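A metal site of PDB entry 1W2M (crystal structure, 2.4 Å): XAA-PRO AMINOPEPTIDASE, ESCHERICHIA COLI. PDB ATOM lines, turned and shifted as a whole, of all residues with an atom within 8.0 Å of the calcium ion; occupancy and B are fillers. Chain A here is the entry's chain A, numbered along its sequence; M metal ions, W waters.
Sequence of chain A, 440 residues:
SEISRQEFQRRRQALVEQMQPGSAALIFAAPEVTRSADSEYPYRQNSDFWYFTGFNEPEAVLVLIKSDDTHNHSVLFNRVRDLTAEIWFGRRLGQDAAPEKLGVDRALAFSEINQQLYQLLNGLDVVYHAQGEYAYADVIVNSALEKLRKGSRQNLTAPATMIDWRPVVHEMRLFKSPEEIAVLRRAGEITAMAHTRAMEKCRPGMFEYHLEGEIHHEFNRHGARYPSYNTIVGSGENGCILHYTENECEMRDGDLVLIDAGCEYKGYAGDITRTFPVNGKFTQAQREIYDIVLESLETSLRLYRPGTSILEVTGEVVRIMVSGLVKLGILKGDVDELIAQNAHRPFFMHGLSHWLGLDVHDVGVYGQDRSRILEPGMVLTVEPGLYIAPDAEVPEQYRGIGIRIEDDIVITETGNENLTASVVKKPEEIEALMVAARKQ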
ATOM      1  N   TYR A 229      26.200   0.974  11.237  1.00  0.00           N
ATOM      2  CA  TYR A 229      24.941   0.366  10.778  1.00  0.00           C
ATOM      3  C   TYR A 229      23.923   1.468  10.543  1.00  0.00           C
ATOM      4  O   TYR A 229      24.143   2.631  10.924  1.00  0.00           O
ATOM      5  CB  TYR A 229      24.374  -0.629  11.823  1.00  0.00           C
ATOM      6  CG  TYR A 229      24.209   0.007  13.165  1.00  0.00           C
ATOM      7  CD1 TYR A 229      25.270   0.142  14.029  1.00  0.00           C
ATOM      8  CD2 TYR A 229      22.982   0.571  13.546  1.00  0.00           C
ATOM      9  CE1 TYR A 229      25.120   0.777  15.295  1.00  0.00           C
ATOM     10  CE2 TYR A 229      22.832   1.211  14.788  1.00  0.00           C
ATOM     11  CZ  TYR A 229      23.901   1.299  15.649  1.00  0.00           C
ATOM     12  OH  TYR A 229      23.743   1.935  16.857  1.00  0.00           O
ATOM     13  N   HIS A 243      14.576  -2.235  14.799  1.00  0.00           N
ATOM     14  CA  HIS A 243      15.454  -1.706  13.735  1.00  0.00           C
ATOM     15  C   HIS A 243      14.647  -0.772  12.793  1.00  0.00           C
ATOM     16  O   HIS A 243      14.724  -0.866  11.575  1.00  0.00           O
ATOM     17  CB  HIS A 243      16.181  -2.826  12.936  1.00  0.00           C
ATOM     18  CG  HIS A 243      17.100  -3.679  13.775  1.00  0.00           C
ATOM     19  ND1 HIS A 243      16.651  -4.709  14.592  1.00  0.00           N
ATOM     20  CD2 HIS A 243      18.458  -3.665  13.908  1.00  0.00           C
ATOM     21  CE1 HIS A 243      17.682  -5.274  15.205  1.00  0.00           C
ATOM     22  NE2 HIS A 243      18.786  -4.667  14.806  1.00  0.00           N
ATOM     23  N   ASP A 260      19.117   4.808  18.049  1.00  0.00           N
ATOM     24  CA  ASP A 260      20.135   3.764  18.025  1.00  0.00           C
ATOM     25  C   ASP A 260      21.062   4.116  16.870  1.00  0.00           C
ATOM     26  O   ASP A 260      20.658   4.069  15.703  1.00  0.00           O
ATOM     27  CB  ASP A 260      19.475   2.423  17.744  1.00  0.00           C
ATOM     28  CG  ASP A 260      20.322   1.239  18.135  1.00  0.00           C
ATOM     29  OD1 ASP A 260      21.579   1.318  18.264  1.00  0.00           O
ATOM     30  OD2 ASP A 260      19.752   0.150  18.341  1.00  0.00           O
ATOM     31  N   GLY A 270      31.092   1.831  17.082  1.00  0.00           N
ATOM     32  CA  GLY A 270      30.396   2.267  18.275  1.00  0.00           C
ATOM     33  C   GLY A 270      28.958   1.837  18.102  1.00  0.00           C
ATOM     34  O   GLY A 270      28.517   1.551  16.990  1.00  0.00           O
ATOM     35  N   ASP A 271      28.227   1.723  19.212  1.00  0.00           N
ATOM     36  CA  ASP A 271      26.835   1.301  19.194  1.00  0.00           C
ATOM     37  C   ASP A 271      26.169   1.784  20.466  1.00  0.00           C
ATOM     38  O   ASP A 271      26.243   1.122  21.506  1.00  0.00           O
ATOM     39  CB  ASP A 271      26.759  -0.226  19.061  1.00  0.00           C
ATOM     40  CG  ASP A 271      25.332  -0.774  18.889  1.00  0.00           C
ATOM     41  OD1 ASP A 271      24.357   0.008  18.771  1.00  0.00           O
ATOM     42  OD2 ASP A 271      25.122  -2.018  18.905  1.00  0.00           O
ATOM     43  N   ILE A 272      25.516   2.943  20.374  1.00  0.00           N
ATOM     44  CA  ILE A 272      24.794   3.536  21.491  1.00  0.00           C
ATOM     45  C   ILE A 272      23.294   3.594  21.203  1.00  0.00           C
ATOM     46  O   ILE A 272      22.862   3.776  20.074  1.00  0.00           O
ATOM     47  CB  ILE A 272      25.322   4.951  21.808  1.00  0.00           C
ATOM     48  CG1 ILE A 272      26.774   4.885  22.319  1.00  0.00           C
ATOM     49  CG2 ILE A 272      24.451   5.658  22.885  1.00  0.00           C
ATOM     50  CD1 ILE A 272      27.373   6.261  22.725  1.00  0.00           C
ATOM     51  N   THR A 273      22.491   3.395  22.256  1.00  0.00           N
ATOM     52  CA  THR A 273      21.096   3.748  22.207  1.00  0.00           C
ATOM     53  C   THR A 273      20.758   4.682  23.380  1.00  0.00           C
ATOM     54  O   THR A 273      21.171   4.459  24.515  1.00  0.00           O
ATOM     55  CB  THR A 273      20.157   2.531  22.253  1.00  0.00           C
ATOM     56  OG1 THR A 273      20.524   1.543  21.282  1.00  0.00           O
ATOM     57  CG2 THR A 273      18.750   2.938  21.821  1.00  0.00           C
ATOM     58  N   HIS A 350      14.640  -9.262  22.842  1.00  0.00           N
ATOM     59  CA  HIS A 350      15.977  -9.459  22.289  1.00  0.00           C
ATOM     60  C   HIS A 350      17.012  -9.704  23.391  1.00  0.00           C
ATOM     61  O   HIS A 350      16.716  -9.607  24.578  1.00  0.00           O
ATOM     62  CB  HIS A 350      16.359  -8.281  21.367  1.00  0.00           C
ATOM     63  CG  HIS A 350      16.367  -6.954  22.049  1.00  0.00           C
ATOM     64  ND1 HIS A 350      17.442  -6.487  22.762  1.00  0.00           N
ATOM     65  CD2 HIS A 350      15.413  -5.985  22.137  1.00  0.00           C
ATOM     66  CE1 HIS A 350      17.161  -5.292  23.253  1.00  0.00           C
ATOM     67  NE2 HIS A 350      15.939  -4.963  22.892  1.00  0.00           N
ATOM     68  N   GLY A 351      18.227 -10.057  22.978  1.00  0.00           N
ATOM     69  CA  GLY A 351      19.333 -10.240  23.891  1.00  0.00           C
ATOM     70  C   GLY A 351      19.794  -8.956  24.569  1.00  0.00           C
ATOM     71  O   GLY A 351      19.592  -7.826  24.063  1.00  0.00           O
ATOM     72  N   LEU A 352      20.423  -9.133  25.722  1.00  0.00           N
ATOM     73  CA  LEU A 352      20.975  -8.033  26.497  1.00  0.00           C
ATOM     74  C   LEU A 352      22.255  -7.504  25.874  1.00  0.00           C
ATOM     75  O   LEU A 352      22.516  -6.317  25.925  1.00  0.00           O
ATOM     76  CB  LEU A 352      21.250  -8.499  27.922  1.00  0.00           C
ATOM     77  CG  LEU A 352      21.771  -7.451  28.914  1.00  0.00           C
ATOM     78  CD1 LEU A 352      20.744  -6.349  29.116  1.00  0.00           C
ATOM     79  CD2 LEU A 352      22.168  -8.092  30.238  1.00  0.00           C
ATOM     80  N   SER A 353      23.061  -8.390  25.289  1.00  0.00           N
ATOM     81  CA  SER A 353      24.430  -8.054  24.891  1.00  0.00           C
ATOM     82  C   SER A 353      24.879  -8.803  23.653  1.00  0.00           C
ATOM     83  O   SER A 353      24.607  -9.995  23.516  1.00  0.00           O
ATOM     84  CB  SER A 353      25.406  -8.396  26.028  1.00  0.00           C
ATOM     85  OG  SER A 353      25.143  -7.622  27.190  1.00  0.00           O
ATOM     86  N   HIS A 354      25.589  -8.104  22.772  1.00  0.00           N
ATOM     87  CA  HIS A 354      26.331  -8.759  21.691  1.00  0.00           C
ATOM     88  C   HIS A 354      27.766  -8.252  21.681  1.00  0.00           C
ATOM     89  O   HIS A 354      28.042  -7.161  22.184  1.00  0.00           O
ATOM     90  CB  HIS A 354      25.625  -8.530  20.342  1.00  0.00           C
ATOM     91  CG  HIS A 354      25.441  -7.098  19.981  1.00  0.00           C
ATOM     92  ND1 HIS A 354      26.476  -6.315  19.492  1.00  0.00           N
ATOM     93  CD2 HIS A 354      24.339  -6.314  19.990  1.00  0.00           C
ATOM     94  CE1 HIS A 354      26.016  -5.099  19.255  1.00  0.00           C
ATOM     95  NE2 HIS A 354      24.731  -5.065  19.564  1.00  0.00           N
ATOM     96  N   TRP A 355      28.669  -9.047  21.125  1.00  0.00           N
ATOM     97  CA  TRP A 355      30.047  -8.655  20.918  1.00  0.00           C
ATOM     98  C   TRP A 355      30.110  -7.468  19.984  1.00  0.00           C
ATOM     99  O   TRP A 355      29.264  -7.310  19.101  1.00  0.00           O
ATOM    100  CB  TRP A 355      30.860  -9.787  20.236  1.00  0.00           C
ATOM    101  CG  TRP A 355      30.800 -11.167  20.867  1.00  0.00           C
ATOM    102  CD1 TRP A 355      30.515 -12.344  20.225  1.00  0.00           C
ATOM    103  CD2 TRP A 355      31.046 -11.511  22.241  1.00  0.00           C
ATOM    104  NE1 TRP A 355      30.566 -13.395  21.107  1.00  0.00           N
ATOM    105  CE2 TRP A 355      30.894 -12.913  22.351  1.00  0.00           C
ATOM    106  CE3 TRP A 355      31.360 -10.773  23.396  1.00  0.00           C
ATOM    107  CZ2 TRP A 355      31.057 -13.586  23.559  1.00  0.00           C
ATOM    108  CZ3 TRP A 355      31.521 -11.455  24.614  1.00  0.00           C
ATOM    109  CH2 TRP A 355      31.359 -12.844  24.685  1.00  0.00           C
ATOM    110  N   LEU A 356      31.159  -6.659  20.136  1.00  0.00           N
ATOM    111  CA  LEU A 356      31.326  -5.455  19.361  1.00  0.00           C
ATOM    112  C   LEU A 356      32.747  -5.392  18.823  1.00  0.00           C
ATOM    113  O   LEU A 356      33.699  -5.761  19.519  1.00  0.00           O
ATOM    114  CB  LEU A 356      31.047  -4.238  20.252  1.00  0.00           C
ATOM    115  CG  LEU A 356      31.059  -2.854  19.604  1.00  0.00           C
ATOM    116  CD1 LEU A 356      29.862  -2.677  18.748  1.00  0.00           C
ATOM    117  CD2 LEU A 356      31.084  -1.756  20.685  1.00  0.00           C
ATOM    118  N   VAL A 360      29.419  -4.529  14.034  1.00  0.00           N
ATOM    119  CA  VAL A 360      28.619  -4.104  15.163  1.00  0.00           C
ATOM    120  C   VAL A 360      28.108  -5.337  15.925  1.00  0.00           C
ATOM    121  O   VAL A 360      28.195  -5.359  17.145  1.00  0.00           O
ATOM    122  CB  VAL A 360      27.469  -3.124  14.764  1.00  0.00           C
ATOM    123  CG1 VAL A 360      26.445  -3.743  13.827  1.00  0.00           C
ATOM    124  CG2 VAL A 360      26.780  -2.594  15.997  1.00  0.00           C
ATOM    125  N   HIS A 361      27.583  -6.324  15.212  1.00  0.00           N
ATOM    126  CA  HIS A 361      27.293  -7.639  15.797  1.00  0.00           C
ATOM    127  C   HIS A 361      28.516  -8.503  15.550  1.00  0.00           C
ATOM    128  O   HIS A 361      28.615  -9.168  14.564  1.00  0.00           O
ATOM    129  CB  HIS A 361      26.029  -8.275  15.184  1.00  0.00           C
ATOM    130  CG  HIS A 361      24.791  -7.505  15.488  1.00  0.00           C
ATOM    131  ND1 HIS A 361      23.667  -7.526  14.684  1.00  0.00           N
ATOM    132  CD2 HIS A 361      24.496  -6.661  16.511  1.00  0.00           C
ATOM    133  CE1 HIS A 361      22.747  -6.741  15.207  1.00  0.00           C
ATOM    134  NE2 HIS A 361      23.227  -6.198  16.311  1.00  0.00           N
ATOM    135  N   LEU A 380      31.637  -5.751  24.413  1.00  0.00           N
ATOM    136  CA  LEU A 380      30.234  -6.048  24.214  1.00  0.00           C
ATOM    137  C   LEU A 380      29.333  -4.872  24.534  1.00  0.00           C
ATOM    138  O   LEU A 380      29.723  -3.924  25.216  1.00  0.00           O
ATOM    139  CB  LEU A 380      29.843  -7.244  25.068  1.00  0.00           C
ATOM    140  CG  LEU A 380      30.105  -7.178  26.588  1.00  0.00           C
ATOM    141  CD1 LEU A 380      29.092  -8.065  27.339  1.00  0.00           C
ATOM    142  CD2 LEU A 380      31.496  -7.588  26.964  1.00  0.00           C
ATOM    143  N   THR A 381      28.114  -4.929  24.025  1.00  0.00           N
ATOM    144  CA  THR A 381      27.099  -3.935  24.335  1.00  0.00           C
ATOM    145  C   THR A 381      26.251  -4.438  25.469  1.00  0.00           C
ATOM    146  O   THR A 381      26.281  -5.610  25.825  1.00  0.00           O
ATOM    147  CB  THR A 381      26.174  -3.692  23.130  1.00  0.00           C
ATOM    148  OG1 THR A 381      25.499  -4.914  22.759  1.00  0.00           O
ATOM    149  CG2 THR A 381      26.980  -3.286  21.887  1.00  0.00           C
ATOM    150  N   VAL A 382      25.543  -3.498  26.078  1.00  0.00           N
ATOM    151  CA  VAL A 382      24.584  -3.766  27.127  1.00  0.00           C
ATOM    152  C   VAL A 382      23.387  -2.938  26.753  1.00  0.00           C
ATOM    153  O   VAL A 382      23.434  -1.704  26.842  1.00  0.00           O
ATOM    154  CB  VAL A 382      25.130  -3.296  28.463  1.00  0.00           C
ATOM    155  CG1 VAL A 382      24.235  -3.736  29.594  1.00  0.00           C
ATOM    156  CG2 VAL A 382      26.566  -3.803  28.645  1.00  0.00           C
ATOM    157  N   GLU A 383      22.316  -3.589  26.340  1.00  0.00           N
ATOM    158  CA  GLU A 383      21.198  -2.877  25.713  1.00  0.00           C
ATOM    159  C   GLU A 383      19.832  -3.359  26.143  1.00  0.00           C
ATOM    160  O   GLU A 383      19.035  -3.815  25.323  1.00  0.00           O
ATOM    161  CB  GLU A 383      21.332  -2.878  24.174  1.00  0.00           C
ATOM    162  CG  GLU A 383      21.432  -4.210  23.494  1.00  0.00           C
ATOM    163  CD  GLU A 383      21.688  -4.100  21.990  1.00  0.00           C
ATOM    164  OE1 GLU A 383      20.953  -3.391  21.270  1.00  0.00           O
ATOM    165  OE2 GLU A 383      22.647  -4.694  21.506  1.00  0.00           O
ATOM    166  N   ARG A 404      14.928   1.876  24.956  1.00  0.00           N
ATOM    167  CA  ARG A 404      16.156   1.113  25.028  1.00  0.00           C
ATOM    168  C   ARG A 404      17.271   2.057  25.408  1.00  0.00           C
ATOM    169  O   ARG A 404      17.276   3.199  24.974  1.00  0.00           O
ATOM    170  CB  ARG A 404      16.433   0.491  23.667  1.00  0.00           C
ATOM    171  CG  ARG A 404      17.802  -0.206  23.570  1.00  0.00           C
ATOM    172  CD  ARG A 404      17.923  -1.216  22.430  1.00  0.00           C
ATOM    173  NE  ARG A 404      17.908  -0.575  21.093  1.00  0.00           N
ATOM    174  CZ  ARG A 404      16.873  -0.558  20.259  1.00  0.00           C
ATOM    175  NH1 ARG A 404      15.714  -1.115  20.563  1.00  0.00           N
ATOM    176  NH2 ARG A 404      17.013   0.014  19.082  1.00  0.00           N
ATOM    177  N   GLU A 406      21.598   1.851  25.789  1.00  0.00           N
ATOM    178  CA  GLU A 406      22.695   0.971  25.437  1.00  0.00           C
ATOM    179  C   GLU A 406      24.061   1.641  25.540  1.00  0.00           C
ATOM    180  O   GLU A 406      24.268   2.725  25.006  1.00  0.00           O
ATOM    181  CB  GLU A 406      22.468   0.468  24.023  1.00  0.00           C
ATOM    182  CG  GLU A 406      23.665  -0.210  23.374  1.00  0.00           C
ATOM    183  CD  GLU A 406      23.387  -0.663  21.953  1.00  0.00           C
ATOM    184  OE1 GLU A 406      22.719   0.073  21.187  1.00  0.00           O
ATOM    185  OE2 GLU A 406      23.852  -1.754  21.595  1.00  0.00           O
ATOM    186  N   ASP A 407      24.971   0.968  26.250  1.00  0.00           N
ATOM    187  CA  ASP A 407      26.370   1.362  26.342  1.00  0.00           C
ATOM    188  C   ASP A 407      27.253   0.260  25.783  1.00  0.00           C
ATOM    189  O   ASP A 407      26.834  -0.881  25.666  1.00  0.00           O
ATOM    190  CB  ASP A 407      26.767   1.572  27.812  1.00  0.00           C
ATOM    191  CG  ASP A 407      26.337   2.898  28.376  1.00  0.00           C
ATOM    192  OD1 ASP A 407      26.165   3.859  27.586  1.00  0.00           O
ATOM    193  OD2 ASP A 407      26.188   3.085  29.623  1.00  0.00           O
ATOM    194  N   ASP A 408      28.498   0.593  25.469  1.00  0.00           N
ATOM    195  CA  ASP A 408      29.513  -0.365  25.045  1.00  0.00           C
ATOM    196  C   ASP A 408      30.559  -0.458  26.135  1.00  0.00           C
ATOM    197  O   ASP A 408      30.996   0.588  26.637  1.00  0.00           O
ATOM    198  CB  ASP A 408      30.168   0.093  23.735  1.00  0.00           C
ATOM    199  CG  ASP A 408      29.166   0.454  22.678  1.00  0.00           C
ATOM    200  OD1 ASP A 408      28.083  -0.193  22.627  1.00  0.00           O
ATOM    201  OD2 ASP A 408      29.392   1.372  21.869  1.00  0.00           O
HETATM  202 CA    CA M   1      23.306  -3.004  19.767  1.00  0.00          CA
HETATM  203  O   HOH W   1      21.810  -1.113  19.338  1.00  0.00           O
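OD1 of Asp 271 is in hydrogen-bond range of OH of Tyr 229. N of Asp 271 lies within hydrogen-bond range of OD2 of Asp 408, 2.9 Å away. The side-chain hydroxyl of Thr 273 is in hydrogen-bond range of the side-chain carboxylate of Glu 406. OG1 of Thr 381 sits close to OE2 of Glu 383. N of Glu 383 lies within hydrogen-bond range of O of Leu 352. The backbone carbonyl oxygen (O) of His 354 lies within hydrogen-bond range of the backbone NH (N) of Thr 381 (2.9 Å). The backbone carbonyl oxygen (O) of Val 360 sits close to a ring nitrogen (ND1) of His 354 (3.1 Å).
Within 4 Å of the calcium ion: Asp 271, His 354, Glu 383 and Glu 406.
The calcium ion is bound by OD2 of Asp 271 (2.2 Å), OE2 of Glu 406 (2.3 Å), water W1 (2.4 Å), OE2 of Glu 383 (2.5 Å), NE2 of His 354 (2.5 Å) and OE1 of Glu 383 (2.8 Å). The calcium ion has six donor atoms within binding distance.
Water W1 bridges the side-chain carboxylate (OD2) of Asp 260 (2.6 Å) and the side-chain carboxylate (OD1) of Asp 271 (2.8 Å).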
